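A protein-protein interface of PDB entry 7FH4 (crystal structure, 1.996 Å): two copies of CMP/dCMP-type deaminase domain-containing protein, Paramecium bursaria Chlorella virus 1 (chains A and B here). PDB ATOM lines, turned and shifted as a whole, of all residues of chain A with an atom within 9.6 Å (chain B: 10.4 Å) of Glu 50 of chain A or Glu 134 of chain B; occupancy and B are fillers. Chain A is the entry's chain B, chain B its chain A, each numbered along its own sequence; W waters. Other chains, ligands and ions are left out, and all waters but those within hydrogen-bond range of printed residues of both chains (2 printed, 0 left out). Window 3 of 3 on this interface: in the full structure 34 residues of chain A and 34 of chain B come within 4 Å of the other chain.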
ATOM      1  N   LYS A  20       1.863  21.324  14.954  1.00  0.00           N
ATOM      2  CA  LYS A  20       2.142  22.678  15.407  1.00  0.00           C
ATOM      3  C   LYS A  20       1.686  23.750  14.421  1.00  0.00           C
ATOM      4  O   LYS A  20       1.880  24.940  14.692  1.00  0.00           O
ATOM      5  CB  LYS A  20       3.644  22.842  15.701  1.00  0.00           C
ATOM      6  CG  LYS A  20       4.194  21.919  16.813  1.00  0.00           C
ATOM      7  CD  LYS A  20       5.544  22.456  17.383  1.00  0.00           C
ATOM      8  CE  LYS A  20       6.346  21.363  18.090  1.00  0.00           C
ATOM      9  NZ  LYS A  20       6.620  20.199  17.187  1.00  0.00           N
ATOM     10  N   GLY A  44       3.930  18.894   9.694  1.00  0.00           N
ATOM     11  CA  GLY A  44       4.895  19.580  10.540  1.00  0.00           C
ATOM     12  C   GLY A  44       6.156  19.868   9.754  1.00  0.00           C
ATOM     13  O   GLY A  44       6.359  19.356   8.647  1.00  0.00           O
ATOM     14  N   LEU A  45       7.001  20.718  10.336  1.00  0.00           N
ATOM     15  CA  LEU A  45       8.282  20.994   9.716  1.00  0.00           C
ATOM     16  C   LEU A  45       9.153  19.738   9.813  1.00  0.00           C
ATOM     17  O   LEU A  45       8.846  18.823  10.577  1.00  0.00           O
ATOM     18  CB  LEU A  45       8.931  22.207  10.379  1.00  0.00           C
ATOM     19  CG  LEU A  45       8.049  23.471  10.475  1.00  0.00           C
ATOM     20  CD1 LEU A  45       8.867  24.693  10.855  1.00  0.00           C
ATOM     21  CD2 LEU A  45       7.272  23.738   9.174  1.00  0.00           C
ATOM     22  N   PRO A  46      10.208  19.631   9.011  1.00  0.00           N
ATOM     23  CA  PRO A  46      11.041  18.427   9.093  1.00  0.00           C
ATOM     24  C   PRO A  46      11.597  18.247  10.499  1.00  0.00           C
ATOM     25  O   PRO A  46      11.793  19.214  11.242  1.00  0.00           O
ATOM     26  CB  PRO A  46      12.150  18.690   8.070  1.00  0.00           C
ATOM     27  CG  PRO A  46      11.521  19.645   7.098  1.00  0.00           C
ATOM     28  CD  PRO A  46      10.679  20.542   7.951  1.00  0.00           C
ATOM     29  N   ARG A  47      11.815  16.988  10.863  1.00  0.00           N
ATOM     30  CA  ARG A  47      12.383  16.630  12.163  1.00  0.00           C
ATOM     31  C   ARG A  47      13.667  17.396  12.442  1.00  0.00           C
ATOM     32  O   ARG A  47      14.624  17.328  11.666  1.00  0.00           O
ATOM     33  CB  ARG A  47      12.643  15.125  12.189  1.00  0.00           C
ATOM     34  CG  ARG A  47      13.257  14.580  13.445  1.00  0.00           C
ATOM     35  CD  ARG A  47      13.310  13.039  13.390  1.00  0.00           C
ATOM     36  NE  ARG A  47      12.025  12.398  13.697  1.00  0.00           N
ATOM     37  CZ  ARG A  47      11.160  11.946  12.785  1.00  0.00           C
ATOM     38  NH1 ARG A  47      11.417  12.065  11.487  1.00  0.00           N
ATOM     39  NH2 ARG A  47      10.029  11.376  13.172  1.00  0.00           N
ATOM     40  N   GLY A  48      13.685  18.131  13.553  1.00  0.00           N
ATOM     41  CA  GLY A  48      14.871  18.851  13.965  1.00  0.00           C
ATOM     42  C   GLY A  48      15.030  20.234  13.372  1.00  0.00           C
ATOM     43  O   GLY A  48      15.984  20.936  13.732  1.00  0.00           O
ATOM     44  N   PHE A  49      14.134  20.648  12.478  1.00  0.00           N
ATOM     45  CA  PHE A  49      14.164  21.992  11.906  1.00  0.00           C
ATOM     46  C   PHE A  49      13.545  22.968  12.903  1.00  0.00           C
ATOM     47  O   PHE A  49      12.391  22.792  13.304  1.00  0.00           O
ATOM     48  CB  PHE A  49      13.401  21.980  10.579  1.00  0.00           C
ATOM     49  CG  PHE A  49      13.691  23.146   9.677  1.00  0.00           C
ATOM     50  CD1 PHE A  49      14.966  23.360   9.184  1.00  0.00           C
ATOM     51  CD2 PHE A  49      12.675  24.000   9.278  1.00  0.00           C
ATOM     52  CE1 PHE A  49      15.228  24.429   8.331  1.00  0.00           C
ATOM     53  CE2 PHE A  49      12.931  25.062   8.421  1.00  0.00           C
ATOM     54  CZ  PHE A  49      14.206  25.276   7.949  1.00  0.00           C
ATOM     55  N   GLU A  50      14.297  23.984  13.333  1.00  0.00           N
ATOM     56  CA  GLU A  50      13.769  24.861  14.377  1.00  0.00           C
ATOM     57  C   GLU A  50      12.461  25.510  13.926  1.00  0.00           C
ATOM     58  O   GLU A  50      12.355  26.020  12.806  1.00  0.00           O
ATOM     59  CB  GLU A  50      14.788  25.927  14.771  1.00  0.00           C
ATOM     60  CG  GLU A  50      14.472  26.535  16.134  1.00  0.00           C
ATOM     61  CD  GLU A  50      15.264  27.781  16.438  1.00  0.00           C
ATOM     62  OE1 GLU A  50      16.305  28.004  15.793  1.00  0.00           O
ATOM     63  OE2 GLU A  50      14.830  28.545  17.324  1.00  0.00           O
ATOM     64  N   GLU A  51      11.451  25.457  14.794  1.00  0.00           N
ATOM     65  CA  GLU A  51      10.092  25.860  14.434  1.00  0.00           C
ATOM     66  C   GLU A  51       9.828  27.251  15.006  1.00  0.00           C
ATOM     67  O   GLU A  51       9.192  27.426  16.043  1.00  0.00           O
ATOM     68  CB  GLU A  51       9.079  24.820  14.923  1.00  0.00           C
ATOM     69  CG  GLU A  51       9.420  23.384  14.478  1.00  0.00           C
ATOM     70  CD  GLU A  51       8.283  22.390  14.675  1.00  0.00           C
ATOM     71  OE1 GLU A  51       7.143  22.674  14.238  1.00  0.00           O
ATOM     72  OE2 GLU A  51       8.537  21.313  15.261  1.00  0.00           O
ATOM     73  N   THR A  52      10.346  28.255  14.313  1.00  0.00           N
ATOM     74  CA  THR A  52      10.138  29.631  14.731  1.00  0.00           C
ATOM     75  C   THR A  52       8.775  30.121  14.254  1.00  0.00           C
ATOM     76  O   THR A  52       8.149  29.534  13.370  1.00  0.00           O
ATOM     77  CB  THR A  52      11.234  30.544  14.179  1.00  0.00           C
ATOM     78  OG1 THR A  52      11.144  30.580  12.749  1.00  0.00           O
ATOM     79  CG2 THR A  52      12.611  30.034  14.583  1.00  0.00           C
ATOM     80  N   SER A  53       8.318  31.223  14.846  1.00  0.00           N
ATOM     81  CA  SER A  53       7.033  31.778  14.434  1.00  0.00           C
ATOM     82  C   SER A  53       7.051  32.166  12.958  1.00  0.00           C
ATOM     83  O   SER A  53       6.068  31.943  12.237  1.00  0.00           O
ATOM     84  CB  SER A  53       6.674  32.974  15.311  1.00  0.00           C
ATOM     85  OG  SER A  53       7.631  33.995  15.160  1.00  0.00           O
ATOM     86  N   ASP A  54       8.176  32.723  12.488  1.00  0.00           N
ATOM     87  CA  ASP A  54       8.304  33.122  11.087  1.00  0.00           C
ATOM     88  C   ASP A  54       8.213  31.929  10.139  1.00  0.00           C
ATOM     89  O   ASP A  54       7.674  32.052   9.035  1.00  0.00           O
ATOM     90  CB  ASP A  54       9.626  33.858  10.864  1.00  0.00           C
ATOM     91  CG  ASP A  54       9.664  35.212  11.541  1.00  0.00           C
ATOM     92  OD1 ASP A  54       8.587  35.820  11.727  1.00  0.00           O
ATOM     93  OD2 ASP A  54      10.773  35.670  11.885  1.00  0.00           O
ATOM     94  N   ARG A  55       8.766  30.776  10.528  1.00  0.00           N
ATOM     95  CA  ARG A  55       8.720  29.614   9.649  1.00  0.00           C
ATOM     96  C   ARG A  55       7.341  28.969   9.603  1.00  0.00           C
ATOM     97  O   ARG A  55       7.048  28.244   8.647  1.00  0.00           O
ATOM     98  CB  ARG A  55       9.766  28.576  10.076  1.00  0.00           C
ATOM     99  CG  ARG A  55      11.209  29.042   9.873  1.00  0.00           C
ATOM    100  CD  ARG A  55      12.225  28.063  10.438  1.00  0.00           C
ATOM    101  NE  ARG A  55      13.564  28.304   9.898  1.00  0.00           N
ATOM    102  CZ  ARG A  55      14.638  27.586  10.204  1.00  0.00           C
ATOM    103  NH1 ARG A  55      14.538  26.580  11.064  1.00  0.00           N
ATOM    104  NH2 ARG A  55      15.813  27.866   9.641  1.00  0.00           N
ATOM    105  N   TRP A  56       6.491  29.216  10.601  1.00  0.00           N
ATOM    106  CA  TRP A  56       5.145  28.663  10.620  1.00  0.00           C
ATOM    107  C   TRP A  56       4.090  29.636  10.107  1.00  0.00           C
ATOM    108  O   TRP A  56       2.930  29.237   9.958  1.00  0.00           O
ATOM    109  CB  TRP A  56       4.761  28.210  12.037  1.00  0.00           C
ATOM    110  CG  TRP A  56       5.032  26.753  12.314  1.00  0.00           C
ATOM    111  CD1 TRP A  56       5.856  26.239  13.279  1.00  0.00           C
ATOM    112  CD2 TRP A  56       4.479  25.623  11.614  1.00  0.00           C
ATOM    113  NE1 TRP A  56       5.850  24.866  13.220  1.00  0.00           N
ATOM    114  CE2 TRP A  56       5.006  24.462  12.218  1.00  0.00           C
ATOM    115  CE3 TRP A  56       3.586  25.482  10.542  1.00  0.00           C
ATOM    116  CZ2 TRP A  56       4.677  23.181  11.779  1.00  0.00           C
ATOM    117  CZ3 TRP A  56       3.262  24.209  10.109  1.00  0.00           C
ATOM    118  CH2 TRP A  56       3.808  23.076  10.727  1.00  0.00           C
ATOM    119  N   TYR A  64       8.529  24.813   3.959  1.00  0.00           N
ATOM    120  CA  TYR A  64       9.116  23.917   4.948  1.00  0.00           C
ATOM    121  C   TYR A  64       8.194  22.804   5.429  1.00  0.00           C
ATOM    122  O   TYR A  64       8.691  21.757   5.852  1.00  0.00           O
ATOM    123  CB  TYR A  64       9.576  24.716   6.174  1.00  0.00           C
ATOM    124  CG  TYR A  64      10.498  25.871   5.866  1.00  0.00           C
ATOM    125  CD1 TYR A  64      11.727  25.662   5.255  1.00  0.00           C
ATOM    126  CD2 TYR A  64      10.156  27.174   6.229  1.00  0.00           C
ATOM    127  CE1 TYR A  64      12.592  26.737   4.997  1.00  0.00           C
ATOM    128  CE2 TYR A  64      11.005  28.243   5.978  1.00  0.00           C
ATOM    129  CZ  TYR A  64      12.220  28.019   5.359  1.00  0.00           C
ATOM    130  OH  TYR A  64      13.055  29.086   5.108  1.00  0.00           O
ATOM    131  N   SER B  99      13.428  17.252  -0.785  1.00  0.00           N
ATOM    132  CA  SER B  99      14.303  17.361   0.382  1.00  0.00           C
ATOM    133  C   SER B  99      13.550  17.045   1.672  1.00  0.00           C
ATOM    134  O   SER B  99      14.114  16.446   2.596  1.00  0.00           O
ATOM    135  CB  SER B  99      14.931  18.758   0.441  1.00  0.00           C
ATOM    136  OG  SER B  99      13.973  19.726   0.821  1.00  0.00           O
ATOM    137  N   ILE B 103      14.617  13.898   4.183  1.00  0.00           N
ATOM    138  CA  ILE B 103      14.822  14.052   5.621  1.00  0.00           C
ATOM    139  C   ILE B 103      13.917  13.101   6.397  1.00  0.00           C
ATOM    140  O   ILE B 103      14.361  12.408   7.320  1.00  0.00           O
ATOM    141  CB  ILE B 103      14.593  15.518   6.028  1.00  0.00           C
ATOM    142  CG1 ILE B 103      15.639  16.401   5.346  1.00  0.00           C
ATOM    143  CG2 ILE B 103      14.617  15.686   7.543  1.00  0.00           C
ATOM    144  CD1 ILE B 103      15.416  17.871   5.553  1.00  0.00           C
ATOM    145  N   SER B 126      17.405  26.502  -2.685  1.00  0.00           N
ATOM    146  CA  SER B 126      17.859  27.257  -1.526  1.00  0.00           C
ATOM    147  C   SER B 126      17.141  26.797  -0.264  1.00  0.00           C
ATOM    148  O   SER B 126      17.750  26.697   0.809  1.00  0.00           O
ATOM    149  CB  SER B 126      17.646  28.751  -1.765  1.00  0.00           C
ATOM    150  OG  SER B 126      17.936  29.489  -0.595  1.00  0.00           O
ATOM    151  N   PHE B 127      15.843  26.500  -0.375  1.00  0.00           N
ATOM    152  CA  PHE B 127      15.113  25.983   0.775  1.00  0.00           C
ATOM    153  C   PHE B 127      15.560  24.564   1.105  1.00  0.00           C
ATOM    154  O   PHE B 127      15.678  24.203   2.285  1.00  0.00           O
ATOM    155  CB  PHE B 127      13.605  26.058   0.517  1.00  0.00           C
ATOM    156  CG  PHE B 127      13.073  27.471   0.463  1.00  0.00           C
ATOM    157  CD1 PHE B 127      13.149  28.299   1.575  1.00  0.00           C
ATOM    158  CD2 PHE B 127      12.500  27.972  -0.700  1.00  0.00           C
ATOM    159  CE1 PHE B 127      12.663  29.608   1.533  1.00  0.00           C
ATOM    160  CE2 PHE B 127      12.013  29.277  -0.753  1.00  0.00           C
ATOM    161  CZ  PHE B 127      12.095  30.095   0.367  1.00  0.00           C
ATOM    162  N   SER B 128      15.852  23.760   0.080  1.00  0.00           N
ATOM    163  CA  SER B 128      16.396  22.421   0.307  1.00  0.00           C
ATOM    164  C   SER B 128      17.656  22.475   1.164  1.00  0.00           C
ATOM    165  O   SER B 128      17.817  21.696   2.112  1.00  0.00           O
ATOM    166  CB  SER B 128      16.706  21.749  -1.029  1.00  0.00           C
ATOM    167  OG  SER B 128      15.526  21.475  -1.743  1.00  0.00           O
ATOM    168  N   ASN B 129      18.567  23.392   0.835  1.00  0.00           N
ATOM    169  CA  ASN B 129      19.853  23.458   1.522  1.00  0.00           C
ATOM    170  C   ASN B 129      19.702  23.967   2.947  1.00  0.00           C
ATOM    171  O   ASN B 129      20.440  23.547   3.847  1.00  0.00           O
ATOM    172  CB  ASN B 129      20.811  24.348   0.735  1.00  0.00           C
ATOM    173  CG  ASN B 129      21.500  23.599  -0.381  1.00  0.00           C
ATOM    174  OD1 ASN B 129      22.007  22.496  -0.172  1.00  0.00           O
ATOM    175  ND2 ASN B 129      21.512  24.183  -1.579  1.00  0.00           N
ATOM    176  N   GLU B 130      18.778  24.899   3.162  1.00  0.00           N
ATOM    177  CA  GLU B 130      18.502  25.361   4.513  1.00  0.00           C
ATOM    178  C   GLU B 130      18.013  24.213   5.393  1.00  0.00           C
ATOM    179  O   GLU B 130      18.468  24.058   6.536  1.00  0.00           O
ATOM    180  CB  GLU B 130      17.478  26.493   4.451  1.00  0.00           C
ATOM    181  CG  GLU B 130      17.300  27.282   5.719  1.00  0.00           C
ATOM    182  CD  GLU B 130      16.122  28.234   5.643  1.00  0.00           C
ATOM    183  OE1 GLU B 130      15.370  28.197   4.629  1.00  0.00           O
ATOM    184  OE2 GLU B 130      15.943  29.008   6.611  1.00  0.00           O
ATOM    185  N   MET B 131      17.102  23.380   4.867  1.00  0.00           N
ATOM    186  CA  MET B 131      16.564  22.260   5.639  1.00  0.00           C
ATOM    187  C   MET B 131      17.602  21.156   5.846  1.00  0.00           C
ATOM    188  O   MET B 131      17.708  20.606   6.948  1.00  0.00           O
ATOM    189  CB  MET B 131      15.305  21.704   4.954  1.00  0.00           C
ATOM    190  CG  MET B 131      14.032  22.505   5.267  1.00  0.00           C
ATOM    191  SD  MET B 131      12.514  21.978   4.416  1.00  0.00           S
ATOM    192  CE  MET B 131      12.994  22.215   2.696  1.00  0.00           C
ATOM    193  N   PHE B 132      18.355  20.802   4.796  1.00  0.00           N
ATOM    194  CA  PHE B 132      19.389  19.768   4.916  1.00  0.00           C
ATOM    195  C   PHE B 132      20.438  20.134   5.970  1.00  0.00           C
ATOM    196  O   PHE B 132      20.814  19.300   6.805  1.00  0.00           O
ATOM    197  CB  PHE B 132      20.075  19.542   3.562  1.00  0.00           C
ATOM    198  CG  PHE B 132      19.268  18.726   2.574  1.00  0.00           C
ATOM    199  CD1 PHE B 132      18.279  17.843   3.000  1.00  0.00           C
ATOM    200  CD2 PHE B 132      19.536  18.825   1.213  1.00  0.00           C
ATOM    201  CE1 PHE B 132      17.559  17.085   2.081  1.00  0.00           C
ATOM    202  CE2 PHE B 132      18.829  18.076   0.285  1.00  0.00           C
ATOM    203  CZ  PHE B 132      17.845  17.188   0.724  1.00  0.00           C
ATOM    204  N   ASP B 133      20.939  21.373   5.934  1.00  0.00           N
ATOM    205  CA  ASP B 133      22.040  21.755   6.819  1.00  0.00           C
ATOM    206  C   ASP B 133      21.603  21.823   8.278  1.00  0.00           C
ATOM    207  O   ASP B 133      22.356  21.440   9.177  1.00  0.00           O
ATOM    208  CB  ASP B 133      22.622  23.098   6.395  1.00  0.00           C
ATOM    209  CG  ASP B 133      23.611  23.624   7.401  1.00  0.00           C
ATOM    210  OD1 ASP B 133      24.755  23.141   7.314  1.00  0.00           O
ATOM    211  OD2 ASP B 133      23.267  24.502   8.241  1.00  0.00           O
ATOM    212  N   GLU B 134      20.402  22.329   8.535  1.00  0.00           N
ATOM    213  CA  GLU B 134      19.911  22.390   9.905  1.00  0.00           C
ATOM    214  C   GLU B 134      19.513  21.008  10.423  1.00  0.00           C
ATOM    215  O   GLU B 134      19.691  20.712  11.609  1.00  0.00           O
ATOM    216  CB  GLU B 134      18.737  23.357   9.975  1.00  0.00           C
ATOM    217  CG  GLU B 134      18.387  23.777  11.366  1.00  0.00           C
ATOM    218  CD  GLU B 134      17.408  24.923  11.393  1.00  0.00           C
ATOM    219  OE1 GLU B 134      17.625  25.933  10.691  1.00  0.00           O
ATOM    220  OE2 GLU B 134      16.412  24.810  12.120  1.00  0.00           O
ATOM    221  N   CYS B 135      18.965  20.149   9.565  1.00  0.00           N
ATOM    222  CA  CYS B 135      18.546  18.818   9.992  1.00  0.00           C
ATOM    223  C   CYS B 135      19.667  17.788   9.916  1.00  0.00           C
ATOM    224  O   CYS B 135      19.442  16.626  10.256  1.00  0.00           O
ATOM    225  CB  CYS B 135      17.351  18.339   9.164  1.00  0.00           C
ATOM    226  SG  CYS B 135      15.893  19.397   9.329  1.00  0.00           S
ATOM    227  N   GLY B 136      20.856  18.178   9.467  1.00  0.00           N
ATOM    228  CA  GLY B 136      21.998  17.293   9.533  1.00  0.00           C
ATOM    229  C   GLY B 136      22.113  16.268   8.431  1.00  0.00           C
ATOM    230  O   GLY B 136      22.675  15.195   8.656  1.00  0.00           O
ATOM    231  N   ILE B 137      21.589  16.559   7.241  1.00  0.00           N
ATOM    232  CA  ILE B 137      21.806  15.717   6.069  1.00  0.00           C
ATOM    233  C   ILE B 137      22.989  16.297   5.303  1.00  0.00           C
ATOM    234  O   ILE B 137      23.020  17.500   5.012  1.00  0.00           O
ATOM    235  CB  ILE B 137      20.538  15.637   5.189  1.00  0.00           C
ATOM    236  CG1 ILE B 137      19.556  14.566   5.693  1.00  0.00           C
ATOM    237  CG2 ILE B 137      20.886  15.260   3.749  1.00  0.00           C
ATOM    238  CD1 ILE B 137      18.926  14.829   7.012  1.00  0.00           C
ATOM    239  N   GLU B 138      23.988  15.461   5.018  1.00  0.00           N
ATOM    240  CA  GLU B 138      25.157  15.933   4.282  1.00  0.00           C
ATOM    241  C   GLU B 138      24.823  16.101   2.808  1.00  0.00           C
ATOM    242  O   GLU B 138      24.005  15.366   2.245  1.00  0.00           O
ATOM    243  CB  GLU B 138      26.334  14.961   4.391  1.00  0.00           C
ATOM    244  CG  GLU B 138      26.776  14.589   5.779  1.00  0.00           C
ATOM    245  CD  GLU B 138      27.889  13.549   5.751  1.00  0.00           C
ATOM    246  OE1 GLU B 138      28.545  13.400   4.692  1.00  0.00           O
ATOM    247  OE2 GLU B 138      28.100  12.875   6.782  1.00  0.00           O
ATOM    248  N   VAL B 139      25.498  17.053   2.176  1.00  0.00           N
ATOM    249  CA  VAL B 139      25.447  17.225   0.731  1.00  0.00           C
ATOM    250  C   VAL B 139      26.861  17.053   0.192  1.00  0.00           C
ATOM    251  O   VAL B 139      27.793  17.689   0.683  1.00  0.00           O
ATOM    252  CB  VAL B 139      24.864  18.599   0.353  1.00  0.00           C
ATOM    253  CG1 VAL B 139      24.961  18.837  -1.146  1.00  0.00           C
ATOM    254  CG2 VAL B 139      23.415  18.699   0.830  1.00  0.00           C
HETATM  255  O   HOH W   1      13.887  30.417   7.758  1.00  0.00           O
HETATM  256  O   HOH W   2      14.000  12.549  10.126  1.00  0.00           O
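The side-chain hydroxyl of Tyr 64 of chain A is in hydrogen-bond range of the side-chain carboxylate of Glu 130 of chain B.
SG of Cys 135 of chain B sits at hydrogen-bond distance from O of Arg 47 of chain A.
The side-chain carboxylate of Glu 134 of chain B lies within salt-bridge range of the guanidinium group of Arg 55 of chain A.
N of Glu 50 of chain A lies within hydrogen-bond range of OE2 of Glu 134 of chain B.
NH2 of Arg 55 of chain A lies within salt-bridge range of OE2 of Glu 130 of chain B, 3.2 Å away.
The backbone carbonyl oxygen of Glu 50 of chain A is in hydrogen-bond range of the guanidinium group of Arg 55 of chain A, 2.8 Å away.
The side-chain hydroxyl of Thr 52 of chain A is in hydrogen-bond range of the backbone NH of Arg 55 of chain A (3.3 Å).
The side-chain sulfur (SG) of Cys 135 of chain B sits close to the backbone carbonyl oxygen (O) of Met 131 of chain B.
Among the printed residues, merely in contact across the chains: Pro 46 of chain A with Ile 103 of chain B (3.9 Å), Pro 46 of chain A with Met 131 of chain B (3.7 Å), Phe 49 of chain A with Glu 130 of chain B (3.7 Å), Phe 49 of chain A with Met 131 of chain B (3.7 Å), Phe 49 of chain A with Glu 134 of chain B (3.5 Å), Phe 49 of chain A with Cys 135 of chain B (3.8 Å), Tyr 64 of chain A with Phe 127 of chain B (3.6 Å) and Tyr 64 of chain A with Met 131 of chain B (3.9 Å).
Leu 45 of chain A touches none of the printed residues of chain B.
No residue of chain B comes within 4 Å of Gly 48 of chain A.
Phe 49 of chain A touches just these residues of chain B: Glu 130, Met 131, Glu 134 and Cys 135.
Glu 50 of chain A touches one residue of chain B.
No residue of chain B comes within 4 Å of Glu 51 of chain A.
No residue of chain B comes within 4 Å of Thr 52 of chain A.
Printed residues of chain B within 4 Å of Arg 55 of chain A: Glu 130 and Glu 134.
Of the printed residues of chain B, Tyr 64 of chain A touches Phe 127 (3.6 Å), Glu 130 (2.5 Å) and Met 131 (3.9 Å).
Ser 99 of chain B touches none of the printed residues of chain A.
Printed residues of chain A within 4 Å of Ile 103 of chain B: Pro 46 (3.9 Å).
No residue of chain A comes within 4 Å of Asp 133 of chain B.
Of the printed residues of chain A, Cys 135 of chain B touches Arg 47 and Phe 49.
The nearest residue of chain B that does not touch Glu 50 of chain A is Cys 135 of chain B (6.3 Å).
The nearest printed residue of chain A that does not touch Cys 135 of chain B is Pro 46 of chain A (4.01 Å).
Of the 16 printed residues of chain B, 6 touch a printed residue of chain A.
Printed residues of chain B that touch a printed residue of chain A: Ile 103, Phe 127, Glu 130, Met 131, Glu 134 and Cys 135.
Hydrophobic or aromatic side chains of chain B within 4 Å of the printed part of chain A: Ile 103, Phe 127 and Met 131.
Of the 15 printed residues of chain A, 6 touch a printed residue of chain B.
Hydrophobic or aromatic side chains of chain A that line the printed part of chain B: Pro 46, Phe 49 and Tyr 64.
Among the printed residues, Asp or Glu carboxylates within 4 Å of a Lys or Arg side-chain nitrogen of the other chain: Arg 55 of chain A with Glu 130 of chain B (3.2 Å) and Arg 55 of chain A with Glu 134 of chain B (2.8 Å).
No position is printed for both chains.
Water W1 lies within hydrogen-bond range of the side-chain carboxylate of Glu 130 of chain B, the guanidinium group of Arg 55 of chain A and the side-chain hydroxyl of Tyr 64 of chain A.
Water W2 bridges the backbone carbonyl oxygen of Ile 103 of chain B and the guanidinium group of Arg 47 of chain A.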
